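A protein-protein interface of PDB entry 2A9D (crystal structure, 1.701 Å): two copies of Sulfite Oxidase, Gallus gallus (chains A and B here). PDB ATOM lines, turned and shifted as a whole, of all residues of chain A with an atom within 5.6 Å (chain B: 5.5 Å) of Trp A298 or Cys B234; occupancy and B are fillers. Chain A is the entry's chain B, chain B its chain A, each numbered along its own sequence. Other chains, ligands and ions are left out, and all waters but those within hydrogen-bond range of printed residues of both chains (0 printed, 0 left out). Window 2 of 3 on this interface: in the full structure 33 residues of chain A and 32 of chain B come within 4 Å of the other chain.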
ATOM      1  N   ASP A 289       7.220  13.768  26.572  1.00  0.00           N
ATOM      2  CA  ASP A 289       7.621  12.504  26.008  1.00  0.00           C
ATOM      3  C   ASP A 289       7.601  12.670  24.497  1.00  0.00           C
ATOM      4  O   ASP A 289       6.675  13.292  23.961  1.00  0.00           O
ATOM      5  CB  ASP A 289       6.650  11.381  26.387  1.00  0.00           C
ATOM      6  CG  ASP A 289       6.635  11.107  27.877  1.00  0.00           C
ATOM      7  OD1 ASP A 289       7.694  11.222  28.515  1.00  0.00           O
ATOM      8  OD2 ASP A 289       5.572  10.737  28.406  1.00  0.00           O
ATOM      9  N   VAL A 290       8.611  12.119  23.832  1.00  0.00           N
ATOM     10  CA  VAL A 290       8.726  12.203  22.376  1.00  0.00           C
ATOM     11  C   VAL A 290       8.991  10.807  21.798  1.00  0.00           C
ATOM     12  O   VAL A 290       9.864  10.069  22.275  1.00  0.00           O
ATOM     13  CB  VAL A 290       9.861  13.158  21.940  1.00  0.00           C
ATOM     14  CG1 VAL A 290       9.975  13.205  20.397  1.00  0.00           C
ATOM     15  CG2 VAL A 290       9.671  14.554  22.520  1.00  0.00           C
ATOM     16  N   SER A 291       8.205  10.449  20.797  1.00  0.00           N
ATOM     17  CA  SER A 291       8.324   9.186  20.102  1.00  0.00           C
ATOM     18  C   SER A 291       8.733   9.408  18.670  1.00  0.00           C
ATOM     19  O   SER A 291       8.408  10.454  18.109  1.00  0.00           O
ATOM     20  CB  SER A 291       6.974   8.480  20.122  1.00  0.00           C
ATOM     21  OG  SER A 291       6.990   7.263  19.398  1.00  0.00           O
ATOM     22  N   ASP A 293       8.411   6.424  16.610  1.00  0.00           N
ATOM     23  CA  ASP A 293       7.763   5.270  16.000  1.00  0.00           C
ATOM     24  C   ASP A 293       6.255   5.316  16.151  1.00  0.00           C
ATOM     25  O   ASP A 293       5.603   4.293  16.384  1.00  0.00           O
ATOM     26  CB  ASP A 293       8.340   3.949  16.557  1.00  0.00           C
ATOM     27  CG  ASP A 293       8.362   3.897  18.078  1.00  0.00           C
ATOM     28  OD1 ASP A 293       7.645   4.698  18.715  1.00  0.00           O
ATOM     29  OD2 ASP A 293       9.115   3.058  18.627  1.00  0.00           O
ATOM     30  N   GLY A 295       4.388   6.545  18.561  1.00  0.00           N
ATOM     31  CA  GLY A 295       3.831   6.415  19.903  1.00  0.00           C
ATOM     32  C   GLY A 295       3.963   5.039  20.525  1.00  0.00           C
ATOM     33  O   GLY A 295       3.308   4.747  21.538  1.00  0.00           O
ATOM     34  N   ARG A 296       4.852   4.221  19.975  1.00  0.00           N
ATOM     35  CA  ARG A 296       5.066   2.877  20.479  1.00  0.00           C
ATOM     36  C   ARG A 296       6.051   2.926  21.638  1.00  0.00           C
ATOM     37  O   ARG A 296       5.839   2.292  22.661  1.00  0.00           O
ATOM     38  CB  ARG A 296       5.673   2.011  19.395  1.00  0.00           C
ATOM     39  CG  ARG A 296       5.060   0.650  19.326  1.00  0.00           C
ATOM     40  CD  ARG A 296       3.951   0.685  18.298  1.00  0.00           C
ATOM     41  NE  ARG A 296       4.502   0.695  16.936  1.00  0.00           N
ATOM     42  CZ  ARG A 296       3.775   0.808  15.822  1.00  0.00           C
ATOM     43  NH1 ARG A 296       2.455   0.987  15.883  1.00  0.00           N
ATOM     44  NH2 ARG A 296       4.378   0.791  14.633  1.00  0.00           N
ATOM     45  N   THR A 297       7.126   3.691  21.457  1.00  0.00           N
ATOM     46  CA  THR A 297       8.160   3.880  22.473  1.00  0.00           C
ATOM     47  C   THR A 297       8.438   5.364  22.577  1.00  0.00           C
ATOM     48  O   THR A 297       8.230   6.114  21.615  1.00  0.00           O
ATOM     49  CB  THR A 297       9.483   3.177  22.132  1.00  0.00           C
ATOM     50  OG1 THR A 297      10.020   3.690  20.912  1.00  0.00           O
ATOM     51  CG2 THR A 297       9.280   1.656  21.995  1.00  0.00           C
ATOM     52  N   TRP A 298       8.962   5.760  23.729  1.00  0.00           N
ATOM     53  CA  TRP A 298       9.142   7.158  24.060  1.00  0.00           C
ATOM     54  C   TRP A 298      10.481   7.458  24.680  1.00  0.00           C
ATOM     55  O   TRP A 298      11.115   6.583  25.269  1.00  0.00           O
ATOM     56  CB  TRP A 298       8.061   7.560  25.073  1.00  0.00           C
ATOM     57  CG  TRP A 298       6.666   7.283  24.595  1.00  0.00           C
ATOM     58  CD1 TRP A 298       5.968   6.126  24.767  1.00  0.00           C
ATOM     59  CD2 TRP A 298       5.819   8.159  23.846  1.00  0.00           C
ATOM     60  NE1 TRP A 298       4.719   6.239  24.213  1.00  0.00           N
ATOM     61  CE2 TRP A 298       4.593   7.476  23.644  1.00  0.00           C
ATOM     62  CE3 TRP A 298       5.950   9.471  23.366  1.00  0.00           C
ATOM     63  CZ2 TRP A 298       3.535   8.032  22.911  1.00  0.00           C
ATOM     64  CZ3 TRP A 298       4.883  10.029  22.675  1.00  0.00           C
ATOM     65  CH2 TRP A 298       3.696   9.313  22.460  1.00  0.00           C
ATOM     66  N   LYS A 299      10.898   8.712  24.515  1.00  0.00           N
ATOM     67  CA  LYS A 299      12.093   9.280  25.107  1.00  0.00           C
ATOM     68  C   LYS A 299      11.662  10.567  25.801  1.00  0.00           C
ATOM     69  O   LYS A 299      10.673  11.172  25.389  1.00  0.00           O
ATOM     70  CB  LYS A 299      13.121   9.612  24.025  1.00  0.00           C
ATOM     71  CG  LYS A 299      13.610   8.384  23.291  1.00  0.00           C
ATOM     72  CD  LYS A 299      14.531   8.709  22.100  1.00  0.00           C
ATOM     73  CE  LYS A 299      15.212   7.435  21.583  1.00  0.00           C
ATOM     74  NZ  LYS A 299      15.873   6.716  22.736  1.00  0.00           N
ATOM     75  N   VAL A 300      12.451  11.038  26.761  1.00  0.00           N
ATOM     76  CA  VAL A 300      12.142  12.267  27.496  1.00  0.00           C
ATOM     77  C   VAL A 300      12.887  13.480  26.925  1.00  0.00           C
ATOM     78  O   VAL A 300      14.128  13.507  26.833  1.00  0.00           O
ATOM     79  CB  VAL A 300      12.452  12.122  29.004  1.00  0.00           C
ATOM     80  CG1 VAL A 300      12.093  13.373  29.769  1.00  0.00           C
ATOM     81  CG2 VAL A 300      11.711  10.902  29.605  1.00  0.00           C
ATOM     82  N   VAL A 334       6.025  11.973  17.571  1.00  0.00           N
ATOM     83  CA  VAL A 334       4.847  12.289  18.376  1.00  0.00           C
ATOM     84  C   VAL A 334       5.335  12.904  19.658  1.00  0.00           C
ATOM     85  O   VAL A 334       6.391  12.501  20.159  1.00  0.00           O
ATOM     86  CB  VAL A 334       4.019  10.991  18.706  1.00  0.00           C
ATOM     87  CG1 VAL A 334       2.666  11.337  19.353  1.00  0.00           C
ATOM     88  CG2 VAL A 334       3.841  10.114  17.455  1.00  0.00           C
ATOM     89  N   CYS A 335       4.637  13.923  20.167  1.00  0.00           N
ATOM     90  CA  CYS A 335       4.978  14.485  21.476  1.00  0.00           C
ATOM     91  C   CYS A 335       3.763  14.553  22.358  1.00  0.00           C
ATOM     92  O   CYS A 335       2.649  14.716  21.858  1.00  0.00           O
ATOM     93  CB  CYS A 335       5.606  15.894  21.354  1.00  0.00           C
ATOM     94  SG  CYS A 335       4.513  17.223  20.798  1.00  0.00           S
ATOM     95  N   LYS A 336       3.964  14.441  23.663  1.00  0.00           N
ATOM     96  CA  LYS A 336       2.845  14.584  24.608  1.00  0.00           C
ATOM     97  C   LYS A 336       3.419  15.112  25.886  1.00  0.00           C
ATOM     98  O   LYS A 336       4.544  14.758  26.267  1.00  0.00           O
ATOM     99  CB  LYS A 336       2.086  13.263  24.826  1.00  0.00           C
ATOM    100  CG  LYS A 336       2.922  12.123  25.400  1.00  0.00           C
ATOM    101  CD  LYS A 336       2.152  10.779  25.408  1.00  0.00           C
ATOM    102  CE  LYS A 336       2.986   9.635  25.919  1.00  0.00           C
ATOM    103  NZ  LYS A 336       3.219   9.714  27.438  1.00  0.00           N
ATOM    104  N   TRP A 363      -2.453  14.002  20.757  1.00  0.00           N
ATOM    105  CA  TRP A 363      -1.030  14.040  20.413  1.00  0.00           C
ATOM    106  C   TRP A 363      -0.787  14.532  18.991  1.00  0.00           C
ATOM    107  O   TRP A 363      -1.478  14.129  18.053  1.00  0.00           O
ATOM    108  CB  TRP A 363      -0.367  12.669  20.510  1.00  0.00           C
ATOM    109  CG  TRP A 363      -0.569  11.878  21.737  1.00  0.00           C
ATOM    110  CD1 TRP A 363      -0.885  12.306  22.992  1.00  0.00           C
ATOM    111  CD2 TRP A 363      -0.426  10.468  21.808  1.00  0.00           C
ATOM    112  NE1 TRP A 363      -0.957  11.222  23.842  1.00  0.00           N
ATOM    113  CE2 TRP A 363      -0.686  10.084  23.127  1.00  0.00           C
ATOM    114  CE3 TRP A 363      -0.110   9.479  20.855  1.00  0.00           C
ATOM    115  CZ2 TRP A 363      -0.674   8.754  23.519  1.00  0.00           C
ATOM    116  CZ3 TRP A 363      -0.067   8.176  21.242  1.00  0.00           C
ATOM    117  CH2 TRP A 363      -0.307   7.821  22.586  1.00  0.00           C
ATOM    118  N   SER B 232       7.971   8.748  32.709  1.00  0.00           N
ATOM    119  CA  SER B 232       7.790   8.372  31.314  1.00  0.00           C
ATOM    120  C   SER B 232       7.630   6.848  31.246  1.00  0.00           C
ATOM    121  O   SER B 232       8.202   6.126  32.079  1.00  0.00           O
ATOM    122  CB  SER B 232       8.997   8.780  30.510  1.00  0.00           C
ATOM    123  OG  SER B 232       8.823   8.511  29.123  1.00  0.00           O
ATOM    124  N   PRO B 233       6.860   6.347  30.261  1.00  0.00           N
ATOM    125  CA  PRO B 233       6.709   4.896  30.116  1.00  0.00           C
ATOM    126  C   PRO B 233       8.021   4.170  29.777  1.00  0.00           C
ATOM    127  O   PRO B 233       8.085   2.956  29.936  1.00  0.00           O
ATOM    128  CB  PRO B 233       5.672   4.753  28.989  1.00  0.00           C
ATOM    129  CG  PRO B 233       5.540   6.039  28.388  1.00  0.00           C
ATOM    130  CD  PRO B 233       6.012   7.093  29.307  1.00  0.00           C
ATOM    131  N   CYS B 234       9.058   4.910  29.390  1.00  0.00           N
ATOM    132  CA  CYS B 234      10.367   4.342  29.049  1.00  0.00           C
ATOM    133  C   CYS B 234      11.201   4.043  30.273  1.00  0.00           C
ATOM    134  O   CYS B 234      12.157   3.275  30.198  1.00  0.00           O
ATOM    135  CB  CYS B 234      11.178   5.298  28.139  1.00  0.00           C
ATOM    136  SG  CYS B 234      11.599   6.987  28.747  1.00  0.00           S
ATOM    137  N   VAL B 235      10.871   4.676  31.391  1.00  0.00           N
ATOM    138  CA  VAL B 235      11.651   4.515  32.618  1.00  0.00           C
ATOM    139  C   VAL B 235      11.446   3.117  33.224  1.00  0.00           C
ATOM    140  O   VAL B 235      10.343   2.610  33.275  1.00  0.00           O
ATOM    141  CB  VAL B 235      11.273   5.613  33.608  1.00  0.00           C
ATOM    142  CG1 VAL B 235      11.809   5.330  35.035  1.00  0.00           C
ATOM    143  CG2 VAL B 235      11.776   6.969  33.098  1.00  0.00           C
ATOM    144  N   ASP B 236      12.531   2.495  33.673  1.00  0.00           N
ATOM    145  CA  ASP B 236      12.437   1.176  34.287  1.00  0.00           C
ATOM    146  C   ASP B 236      13.195   1.256  35.604  1.00  0.00           C
ATOM    147  O   ASP B 236      13.738   2.297  35.950  1.00  0.00           O
ATOM    148  CB  ASP B 236      13.029   0.085  33.387  1.00  0.00           C
ATOM    149  CG  ASP B 236      12.566  -1.332  33.776  1.00  0.00           C
ATOM    150  OD1 ASP B 236      11.844  -1.538  34.766  1.00  0.00           O
ATOM    151  OD2 ASP B 236      12.961  -2.265  33.078  1.00  0.00           O
ATOM    152  N   THR B 239      16.721   2.828  35.776  1.00  0.00           N
ATOM    153  CA  THR B 239      16.883   4.240  35.408  1.00  0.00           C
ATOM    154  C   THR B 239      16.067   5.244  36.188  1.00  0.00           C
ATOM    155  O   THR B 239      16.333   6.443  36.095  1.00  0.00           O
ATOM    156  CB  THR B 239      16.558   4.452  33.920  1.00  0.00           C
ATOM    157  OG1 THR B 239      15.199   4.085  33.669  1.00  0.00           O
ATOM    158  CG2 THR B 239      17.505   3.589  33.080  1.00  0.00           C
ATOM    159  N   ALA B 350      -0.877   1.912  27.632  1.00  0.00           N
ATOM    160  CA  ALA B 350       0.561   1.787  27.410  1.00  0.00           C
ATOM    161  C   ALA B 350       1.325   3.132  27.436  1.00  0.00           C
ATOM    162  O   ALA B 350       2.414   3.192  27.970  1.00  0.00           O
ATOM    163  CB  ALA B 350       0.888   1.043  26.113  1.00  0.00           C
ATOM    164  N   PRO B 351       0.789   4.170  26.789  1.00  0.00           N
ATOM    165  CA  PRO B 351       1.497   5.447  26.792  1.00  0.00           C
ATOM    166  C   PRO B 351       1.546   6.188  28.145  1.00  0.00           C
ATOM    167  O   PRO B 351       2.372   7.086  28.282  1.00  0.00           O
ATOM    168  CB  PRO B 351       0.720   6.282  25.769  1.00  0.00           C
ATOM    169  CG  PRO B 351      -0.112   5.290  24.982  1.00  0.00           C
ATOM    170  CD  PRO B 351      -0.442   4.251  25.982  1.00  0.00           C
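The side-chain hydroxyl (OG) of Ser B232 is in hydrogen-bond range of the side-chain carboxylate (OD1) of Asp A289 (3.0 Å).
O of Trp A298 lies close to SG of Cys B234 (3.5 Å).
The side-chain amino group of Lys A336 sits at hydrogen-bond distance from the backbone carbonyl oxygen of Pro B351, 2.9 Å away.
SG of Cys B234 sits at hydrogen-bond distance from OG of Ser B232 (3.2 Å).
OD2 of Asp A289 is in salt-bridge range of NZ of Lys A336 (2.7 Å).
The indole nitrogen (NE1) of Trp A298 lies within hydrogen-bond range of the backbone carbonyl oxygen (O) of Gly A295 (3.4 Å).
Among the printed residues, pairs that only touch across the chains: Trp A363 with Pro B351, Val A300 with Ser B232, Trp A298 with Pro B233 and Asp A289 with Pro B233.
Gly A295 touches none of the printed residues of chain B.
Of chain B, only Pro B233 (3.6 Å) and Cys B234 (3.1 Å) come within 4 Å of Trp A298.
Printed residues of chain B within 4 Å of Val A300: Ser B232.
Printed residues of chain B within 4 Å of Lys A336: Pro B351.
Printed residues of chain B within 4 Å of Trp A363: Pro B351.
Printed residues of chain A within 4 Å of Ser B232: Asp A289 and Val A300.
Of the printed residues of chain A, Cys B234 touches Trp A298 (3.1 Å).
Thr B239 touches none of the printed residues of chain A.
The nearest printed residue of chain A that does not touch Cys B234 is Val A300 (4.01 Å).
Of the 14 printed residues of chain A, 5 touch a printed residue of chain B.
Hydrophobic or aromatic side chains of chain A within 4 Å of the printed part of chain B: Trp A298, Val A300 and Trp A363.
Among the printed residues, 7 pairs touch across the chains.
Among the printed residues, no Asp or Glu carboxylate lies within 4 Å of a Lys or Arg side-chain nitrogen of the other chain.
No position is printed for both chains.
Of the 7 pairs that touch across the chains among the printed residues, none has its exchanged pair printed and touching as well.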
